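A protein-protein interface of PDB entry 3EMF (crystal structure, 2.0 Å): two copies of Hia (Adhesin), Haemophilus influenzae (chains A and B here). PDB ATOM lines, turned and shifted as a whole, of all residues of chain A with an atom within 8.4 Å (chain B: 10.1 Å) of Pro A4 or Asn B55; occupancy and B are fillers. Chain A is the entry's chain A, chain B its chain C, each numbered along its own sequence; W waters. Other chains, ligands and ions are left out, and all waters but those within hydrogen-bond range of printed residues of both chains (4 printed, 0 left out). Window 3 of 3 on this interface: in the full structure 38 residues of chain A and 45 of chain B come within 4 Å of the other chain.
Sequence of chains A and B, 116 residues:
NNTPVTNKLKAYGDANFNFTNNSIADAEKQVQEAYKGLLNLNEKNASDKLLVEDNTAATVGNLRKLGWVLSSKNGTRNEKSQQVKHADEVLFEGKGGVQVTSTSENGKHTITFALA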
ATOM      1  N   THR A   3      -4.051   9.725 -24.864  1.00  0.00           N
ATOM      2  CA  THR A   3      -5.359  10.356 -24.863  1.00  0.00           C
ATOM      3  C   THR A   3      -5.294  11.863 -25.036  1.00  0.00           C
ATOM      4  O   THR A   3      -4.564  12.541 -24.309  1.00  0.00           O
ATOM      5  N   PRO A   4      -6.049  12.396 -26.016  1.00  0.00           N
ATOM      6  CA  PRO A   4      -6.138  13.837 -26.292  1.00  0.00           C
ATOM      7  C   PRO A   4      -7.112  14.550 -25.352  1.00  0.00           C
ATOM      8  O   PRO A   4      -8.311  14.578 -25.623  1.00  0.00           O
ATOM      9  CB  PRO A   4      -6.679  13.894 -27.730  1.00  0.00           C
ATOM     10  CG  PRO A   4      -6.613  12.477 -28.252  1.00  0.00           C
ATOM     11  CD  PRO A   4      -6.740  11.606 -27.045  1.00  0.00           C
ATOM     12  N   VAL A   5      -6.597  15.118 -24.267  1.00  0.00           N
ATOM     13  CA  VAL A   5      -7.432  15.815 -23.298  1.00  0.00           C
ATOM     14  C   VAL A   5      -7.591  17.275 -23.696  1.00  0.00           C
ATOM     15  O   VAL A   5      -6.612  17.955 -24.008  1.00  0.00           O
ATOM     16  CB  VAL A   5      -6.819  15.753 -21.881  1.00  0.00           C
ATOM     17  CG1 VAL A   5      -7.604  16.633 -20.910  1.00  0.00           C
ATOM     18  CG2 VAL A   5      -6.749  14.315 -21.390  1.00  0.00           C
ATOM     19  N   THR A   6      -8.828  17.757 -23.670  1.00  0.00           N
ATOM     20  CA  THR A   6      -9.116  19.149 -23.997  1.00  0.00           C
ATOM     21  C   THR A   6     -10.116  19.748 -23.010  1.00  0.00           C
ATOM     22  O   THR A   6     -10.801  19.026 -22.303  1.00  0.00           O
ATOM     23  CB  THR A   6      -9.695  19.280 -25.419  1.00  0.00           C
ATOM     24  OG1 THR A   6     -11.017  18.716 -25.461  1.00  0.00           O
ATOM     25  CG2 THR A   6      -8.806  18.558 -26.421  1.00  0.00           C
ATOM     26  N   ASN A   7     -10.174  21.073 -22.952  1.00  0.00           N
ATOM     27  CA  ASN A   7     -11.261  21.743 -22.255  1.00  0.00           C
ATOM     28  C   ASN A   7     -11.622  23.030 -22.988  1.00  0.00           C
ATOM     29  O   ASN A   7     -11.018  23.342 -24.012  1.00  0.00           O
ATOM     30  CB  ASN A   7     -10.950  21.947 -20.757  1.00  0.00           C
ATOM     31  CG  ASN A   7      -9.753  22.835 -20.513  1.00  0.00           C
ATOM     32  OD1 ASN A   7      -9.524  23.792 -21.249  1.00  0.00           O
ATOM     33  ND2 ASN A   7      -8.987  22.530 -19.463  1.00  0.00           N
ATOM     34  N   ALA A  58      -7.186  19.840 -16.291  1.00  0.00           N
ATOM     35  CA  ALA A  58      -6.345  20.900 -16.826  1.00  0.00           C
ATOM     36  C   ALA A  58      -5.422  20.286 -17.883  1.00  0.00           C
ATOM     37  O   ALA A  58      -5.047  19.118 -17.789  1.00  0.00           O
ATOM     38  CB  ALA A  58      -5.535  21.556 -15.734  1.00  0.00           C
ATOM     39  N   THR A  59      -5.089  21.055 -18.908  1.00  0.00           N
ATOM     40  CA  THR A  59      -4.194  20.558 -19.962  1.00  0.00           C
ATOM     41  C   THR A  59      -2.837  21.251 -19.919  1.00  0.00           C
ATOM     42  O   THR A  59      -2.688  22.304 -19.306  1.00  0.00           O
ATOM     43  CB  THR A  59      -4.792  20.779 -21.358  1.00  0.00           C
ATOM     44  OG1 THR A  59      -4.745  22.175 -21.667  1.00  0.00           O
ATOM     45  CG2 THR A  59      -6.237  20.279 -21.392  1.00  0.00           C
ATOM     46  N   VAL A  60      -1.855  20.659 -20.582  1.00  0.00           N
ATOM     47  CA  VAL A  60      -0.545  21.289 -20.702  1.00  0.00           C
ATOM     48  C   VAL A  60      -0.687  22.601 -21.467  1.00  0.00           C
ATOM     49  O   VAL A  60      -0.035  23.572 -21.138  1.00  0.00           O
ATOM     50  CB  VAL A  60       0.482  20.345 -21.367  1.00  0.00           C
ATOM     51  CG1 VAL A  60       1.833  21.055 -21.565  1.00  0.00           C
ATOM     52  CG2 VAL A  60       0.638  19.070 -20.511  1.00  0.00           C
ATOM     53  N   GLY A  61      -1.568  22.648 -22.470  1.00  0.00           N
ATOM     54  CA  GLY A  61      -1.854  23.909 -23.116  1.00  0.00           C
ATOM     55  C   GLY A  61      -2.295  24.999 -22.139  1.00  0.00           C
ATOM     56  O   GLY A  61      -1.953  26.177 -22.300  1.00  0.00           O
ATOM     57  N   ASN A  62      -3.067  24.616 -21.129  1.00  0.00           N
ATOM     58  CA  ASN A  62      -3.493  25.558 -20.098  1.00  0.00           C
ATOM     59  C   ASN A  62      -2.286  26.103 -19.324  1.00  0.00           C
ATOM     60  O   ASN A  62      -2.203  27.295 -19.053  1.00  0.00           O
ATOM     61  CB  ASN A  62      -4.447  24.896 -19.098  1.00  0.00           C
ATOM     62  CG  ASN A  62      -5.795  24.503 -19.691  1.00  0.00           C
ATOM     63  OD1 ASN A  62      -6.260  25.050 -20.701  1.00  0.00           O
ATOM     64  ND2 ASN A  62      -6.449  23.535 -19.033  1.00  0.00           N
ATOM     65  N   ARG A  64       0.578  26.575 -20.310  1.00  0.00           N
ATOM     66  CA  ARG A  64       1.361  27.438 -21.173  1.00  0.00           C
ATOM     67  C   ARG A  64       0.753  28.830 -21.239  1.00  0.00           C
ATOM     68  O   ARG A  64       1.352  29.744 -21.781  1.00  0.00           O
ATOM     69  CB  ARG A  64       1.491  26.839 -22.577  1.00  0.00           C
ATOM     70  CG  ARG A  64       2.271  25.530 -22.602  1.00  0.00           C
ATOM     71  CD  ARG A  64       2.492  25.005 -24.004  1.00  0.00           C
ATOM     72  NE  ARG A  64       3.468  23.922 -23.983  1.00  0.00           N
ATOM     73  CZ  ARG A  64       3.262  22.713 -24.483  1.00  0.00           C
ATOM     74  NH1 ARG A  64       2.113  22.424 -25.084  1.00  0.00           N
ATOM     75  NH2 ARG A  64       4.212  21.795 -24.395  1.00  0.00           N
ATOM     76  N   LYS A  65      -0.441  28.985 -20.680  1.00  0.00           N
ATOM     77  CA  LYS A  65      -1.119  30.276 -20.709  1.00  0.00           C
ATOM     78  C   LYS A  65      -1.273  30.889 -19.324  1.00  0.00           C
ATOM     79  O   LYS A  65      -1.931  31.915 -19.161  1.00  0.00           O
ATOM     80  CB  LYS A  65      -2.492  30.142 -21.362  1.00  0.00           C
ATOM     81  CG  LYS A  65      -2.442  29.682 -22.798  1.00  0.00           C
ATOM     82  CD  LYS A  65      -3.833  29.817 -23.415  1.00  0.00           C
ATOM     83  CE  LYS A  65      -3.795  29.513 -24.913  1.00  0.00           C
ATOM     84  NZ  LYS A  65      -3.277  28.140 -25.194  1.00  0.00           N
ATOM     85  N   VAL B   5      -2.334   9.701 -13.931  1.00  0.00           N
ATOM     86  CA  VAL B   5      -2.083  10.402 -15.185  1.00  0.00           C
ATOM     87  C   VAL B   5      -0.608  10.738 -15.295  1.00  0.00           C
ATOM     88  O   VAL B   5       0.034  11.055 -14.299  1.00  0.00           O
ATOM     89  CB  VAL B   5      -2.912  11.711 -15.264  1.00  0.00           C
ATOM     90  CG1 VAL B   5      -2.258  12.728 -16.188  1.00  0.00           C
ATOM     91  CG2 VAL B   5      -4.338  11.422 -15.712  1.00  0.00           C
ATOM     92  N   THR B   6      -0.071  10.673 -16.506  1.00  0.00           N
ATOM     93  CA  THR B   6       1.329  11.010 -16.733  1.00  0.00           C
ATOM     94  C   THR B   6       1.534  11.776 -18.040  1.00  0.00           C
ATOM     95  O   THR B   6       0.701  11.725 -18.942  1.00  0.00           O
ATOM     96  CB  THR B   6       2.214   9.746 -16.764  1.00  0.00           C
ATOM     97  OG1 THR B   6       1.745   8.858 -17.786  1.00  0.00           O
ATOM     98  CG2 THR B   6       2.173   9.030 -15.423  1.00  0.00           C
ATOM     99  N   ASN B   7       2.645  12.499 -18.122  1.00  0.00           N
ATOM    100  CA  ASN B   7       3.101  13.065 -19.386  1.00  0.00           C
ATOM    101  C   ASN B   7       4.629  13.142 -19.445  1.00  0.00           C
ATOM    102  O   ASN B   7       5.310  12.770 -18.489  1.00  0.00           O
ATOM    103  CB  ASN B   7       2.434  14.418 -19.680  1.00  0.00           C
ATOM    104  CG  ASN B   7       2.774  15.484 -18.659  1.00  0.00           C
ATOM    105  OD1 ASN B   7       3.937  15.646 -18.275  1.00  0.00           O
ATOM    106  ND2 ASN B   7       1.759  16.247 -18.236  1.00  0.00           N
ATOM    107  N   LEU B  50       6.686  20.337 -30.430  1.00  0.00           N
ATOM    108  CA  LEU B  50       6.635  20.299 -28.970  1.00  0.00           C
ATOM    109  C   LEU B  50       6.647  18.848 -28.533  1.00  0.00           C
ATOM    110  O   LEU B  50       5.926  18.034 -29.100  1.00  0.00           O
ATOM    111  CB  LEU B  50       5.368  20.973 -28.450  1.00  0.00           C
ATOM    112  CG  LEU B  50       5.331  22.491 -28.542  1.00  0.00           C
ATOM    113  CD1 LEU B  50       3.894  22.976 -28.336  1.00  0.00           C
ATOM    114  CD2 LEU B  50       6.262  23.101 -27.517  1.00  0.00           C
ATOM    115  N   LEU B  51       7.472  18.533 -27.537  1.00  0.00           N
ATOM    116  CA  LEU B  51       7.514  17.197 -26.945  1.00  0.00           C
ATOM    117  C   LEU B  51       6.137  16.760 -26.427  1.00  0.00           C
ATOM    118  O   LEU B  51       5.709  15.627 -26.652  1.00  0.00           O
ATOM    119  CB  LEU B  51       8.532  17.161 -25.800  1.00  0.00           C
ATOM    120  CG  LEU B  51       8.600  15.873 -24.973  1.00  0.00           C
ATOM    121  CD1 LEU B  51       8.948  14.677 -25.869  1.00  0.00           C
ATOM    122  CD2 LEU B  51       9.597  16.008 -23.836  1.00  0.00           C
ATOM    123  N   VAL B  52       5.462  17.667 -25.723  1.00  0.00           N
ATOM    124  CA  VAL B  52       4.113  17.419 -25.214  1.00  0.00           C
ATOM    125  C   VAL B  52       3.126  18.411 -25.829  1.00  0.00           C
ATOM    126  O   VAL B  52       3.274  19.613 -25.671  1.00  0.00           O
ATOM    127  CB  VAL B  52       4.072  17.572 -23.693  1.00  0.00           C
ATOM    128  CG1 VAL B  52       2.663  17.274 -23.159  1.00  0.00           C
ATOM    129  CG2 VAL B  52       5.114  16.675 -23.060  1.00  0.00           C
ATOM    130  N   GLU B  53       2.116  17.903 -26.535  1.00  0.00           N
ATOM    131  CA  GLU B  53       1.159  18.772 -27.201  1.00  0.00           C
ATOM    132  C   GLU B  53       0.220  19.460 -26.207  1.00  0.00           C
ATOM    133  O   GLU B  53      -0.014  18.957 -25.105  1.00  0.00           O
ATOM    134  CB  GLU B  53       0.331  17.969 -28.217  1.00  0.00           C
ATOM    135  CG  GLU B  53       1.058  16.792 -28.860  1.00  0.00           C
ATOM    136  CD  GLU B  53       0.863  15.483 -28.099  1.00  0.00           C
ATOM    137  OE1 GLU B  53       1.479  15.316 -27.020  1.00  0.00           O
ATOM    138  OE2 GLU B  53       0.102  14.616 -28.593  1.00  0.00           O
ATOM    139  N   ASP B  54      -0.340  20.593 -26.623  1.00  0.00           N
ATOM    140  CA  ASP B  54      -1.322  21.337 -25.829  1.00  0.00           C
ATOM    141  C   ASP B  54      -2.417  20.452 -25.212  1.00  0.00           C
ATOM    142  O   ASP B  54      -2.748  20.592 -24.025  1.00  0.00           O
ATOM    143  CB  ASP B  54      -1.977  22.436 -26.681  1.00  0.00           C
ATOM    144  CG  ASP B  54      -1.050  23.619 -26.945  1.00  0.00           C
ATOM    145  OD1 ASP B  54      -0.013  23.754 -26.253  1.00  0.00           O
ATOM    146  OD2 ASP B  54      -1.371  24.429 -27.843  1.00  0.00           O
ATOM    147  N   ASN B  55      -2.982  19.548 -26.012  1.00  0.00           N
ATOM    148  CA  ASN B  55      -4.125  18.755 -25.552  1.00  0.00           C
ATOM    149  C   ASN B  55      -3.714  17.488 -24.826  1.00  0.00           C
ATOM    150  O   ASN B  55      -4.083  16.380 -25.203  1.00  0.00           O
ATOM    151  CB  ASN B  55      -5.091  18.448 -26.701  1.00  0.00           C
ATOM    152  CG  ASN B  55      -5.666  19.706 -27.320  1.00  0.00           C
ATOM    153  OD1 ASN B  55      -5.922  20.694 -26.625  1.00  0.00           O
ATOM    154  ND2 ASN B  55      -5.869  19.679 -28.639  1.00  0.00           N
ATOM    155  N   THR B  56      -2.934  17.675 -23.773  1.00  0.00           N
ATOM    156  CA  THR B  56      -2.482  16.584 -22.937  1.00  0.00           C
ATOM    157  C   THR B  56      -2.829  16.950 -21.513  1.00  0.00           C
ATOM    158  O   THR B  56      -2.700  18.107 -21.124  1.00  0.00           O
ATOM    159  CB  THR B  56      -0.960  16.421 -23.041  1.00  0.00           C
ATOM    160  OG1 THR B  56      -0.597  16.190 -24.413  1.00  0.00           O
ATOM    161  CG2 THR B  56      -0.478  15.251 -22.186  1.00  0.00           C
ATOM    162  N   ALA B  57      -3.274  15.974 -20.732  1.00  0.00           N
ATOM    163  CA  ALA B  57      -3.568  16.229 -19.325  1.00  0.00           C
ATOM    164  C   ALA B  57      -2.336  16.731 -18.572  1.00  0.00           C
ATOM    165  O   ALA B  57      -1.223  16.229 -18.768  1.00  0.00           O
ATOM    166  CB  ALA B  57      -4.139  14.980 -18.656  1.00  0.00           C
ATOM    167  N   ALA B  58      -2.547  17.744 -17.736  1.00  0.00           N
ATOM    168  CA  ALA B  58      -1.528  18.225 -16.806  1.00  0.00           C
ATOM    169  C   ALA B  58      -1.572  17.409 -15.504  1.00  0.00           C
ATOM    170  O   ALA B  58      -2.611  16.878 -15.129  1.00  0.00           O
ATOM    171  CB  ALA B  58      -1.746  19.720 -16.504  1.00  0.00           C
HETATM  172  O   HOH W   1       6.897  20.246 -24.521  1.00  0.00           O
HETATM  173  O   HOH W   2      -5.426  22.783 -24.111  1.00  0.00           O
HETATM  174  O   HOH W   3      -5.464  16.929 -15.840  1.00  0.00           O
HETATM  175  O   HOH W   4      -3.318  12.940 -21.768  1.00  0.00           O
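The backbone NH (N) of Gly A61 lies within hydrogen-bond range of the backbone carbonyl oxygen (O) of Asp B54, at 2.8 Å. The backbone carbonyl oxygen (O) of Thr B56 lies within hydrogen-bond range of the backbone NH (N) of Val A60. The backbone carbonyl oxygen of Asp B54 lies close to the side-chain hydroxyl of Thr A59, at 3.5 Å. The side-chain carboxylate (OD1) of Asp B54 lies within salt-bridge range of the guanidinium group (NH1) of Arg A64 (2.8 Å). N of Val A5 is in hydrogen-bond range of O of Asn B55, 3.0 Å away. The guanidinium group of Arg A64 lies within hydrogen-bond range of the backbone carbonyl oxygen of Val B52. O of Ala A58 is in hydrogen-bond range of N of Ala B58, 2.9 Å away.
Printed residues of chain B that touch a printed residue of chain A: Asn B7, Leu B50, Val B52, Glu B53, Asp B54, Asn B55, Thr B56, Ala B57 and Ala B58. Hydrophobic or aromatic side chains of chain B that line the printed part of chain A: Leu B50, Val B52, Ala B57 and Ala B58. Hydrophobic or aromatic side chains of chain A that line the printed part of chain B: Val A5 and Val A60. Along chain A the printed residues that touch a printed residue of chain B span positions 3 to 64. Among the printed residues, 21 pairs touch across the chains. Among the printed residues, Asp or Glu carboxylates within 4 Å of a Lys or Arg side-chain nitrogen of the other chain: Arg A64 with Asp B54 (2.8 Å).
Among the printed residues, pairs that only touch across the chains: Thr A59 with Thr B56 (3.1 Å), Pro A4 with Asn B55 (3.4 Å), Thr A6 with Asn B55 (3.5 Å), Val A60 with Asp B54 (3.6 Å), Ala A58 with Ala B57 (3.6 Å), Arg A64 with Glu B53 (3.7 Å), Val A5 with Thr B56 (3.7 Å), Val A5 with Ala B57 (3.7 Å), Arg A64 with Leu B50 (3.7 Å), Val A60 with Val B52 (3.8 Å), Val A60 with Asn B7 (3.8 Å), Val A60 with Ala B57 (3.8 Å), Thr A59 with Ala B58 (3.9 Å) and Thr A3 with Asn B55 (3.97 Å).
Ala A58 touches its own counterpart, Ala B58. Positions printed for both chains: 5, 6, 7 and 58.
Water W2 lies within hydrogen-bond range of the side-chain hydroxyl (OG1) of Thr A59 (2.6 Å), the side-chain amide oxygen (OD1) of Asn B55 (3.3 Å) and the backbone carbonyl oxygen (O) of Asp B54 (3.5 Å). Water W4 bridges the backbone carbonyl oxygen of Thr A3 (2.9 Å) and the backbone NH of Ala B57 (3.2 Å). Water W3 lies within hydrogen-bond range of the backbone carbonyl oxygen of Ala B58 and the backbone carbonyl oxygen of Ala A58. Water W1 bridges the guanidinium group of Arg A64 (3.1 Å) and the backbone NH of Val B52 (3.2 Å).
Pro A4 touches just one residue of chain B: Asn B55. Asn B55 touches just these residues of chain A: Thr A3, Pro A4, Val A5 and Thr A6. Of the printed residues of chain B, Thr A3 touches Asn B55 (3.97 Å). Of the printed residues of chain B, Arg A64 touches Leu B50, Val B52, Glu B53 and Asp B54. Printed residues of chain B within 4 Å of Val A60: Asn B7, Val B52, Asp B54, Thr B56 and Ala B57. Printed residues of chain A within 4 Å of Asp B54: Thr A59, Val A60, Gly A61 and Arg A64. Lys A65 touches none of the printed residues of chain B. The nearest residue of chain B that does not touch Pro A4 is Thr B56 (5.5 Å).
OG1 of Thr A59 lies close to N of Gly A61 (3.3 Å). N of Thr A59 lies close to ND2 of Asn A62. The side-chain amide nitrogen of Asn B7 sits at hydrogen-bond distance from the backbone carbonyl oxygen of Ala B57, 3.0 Å away. The backbone carbonyl oxygen (O) of Glu B53 sits at hydrogen-bond distance from the side-chain hydroxyl (OG1) of Thr B56 (2.9 Å).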
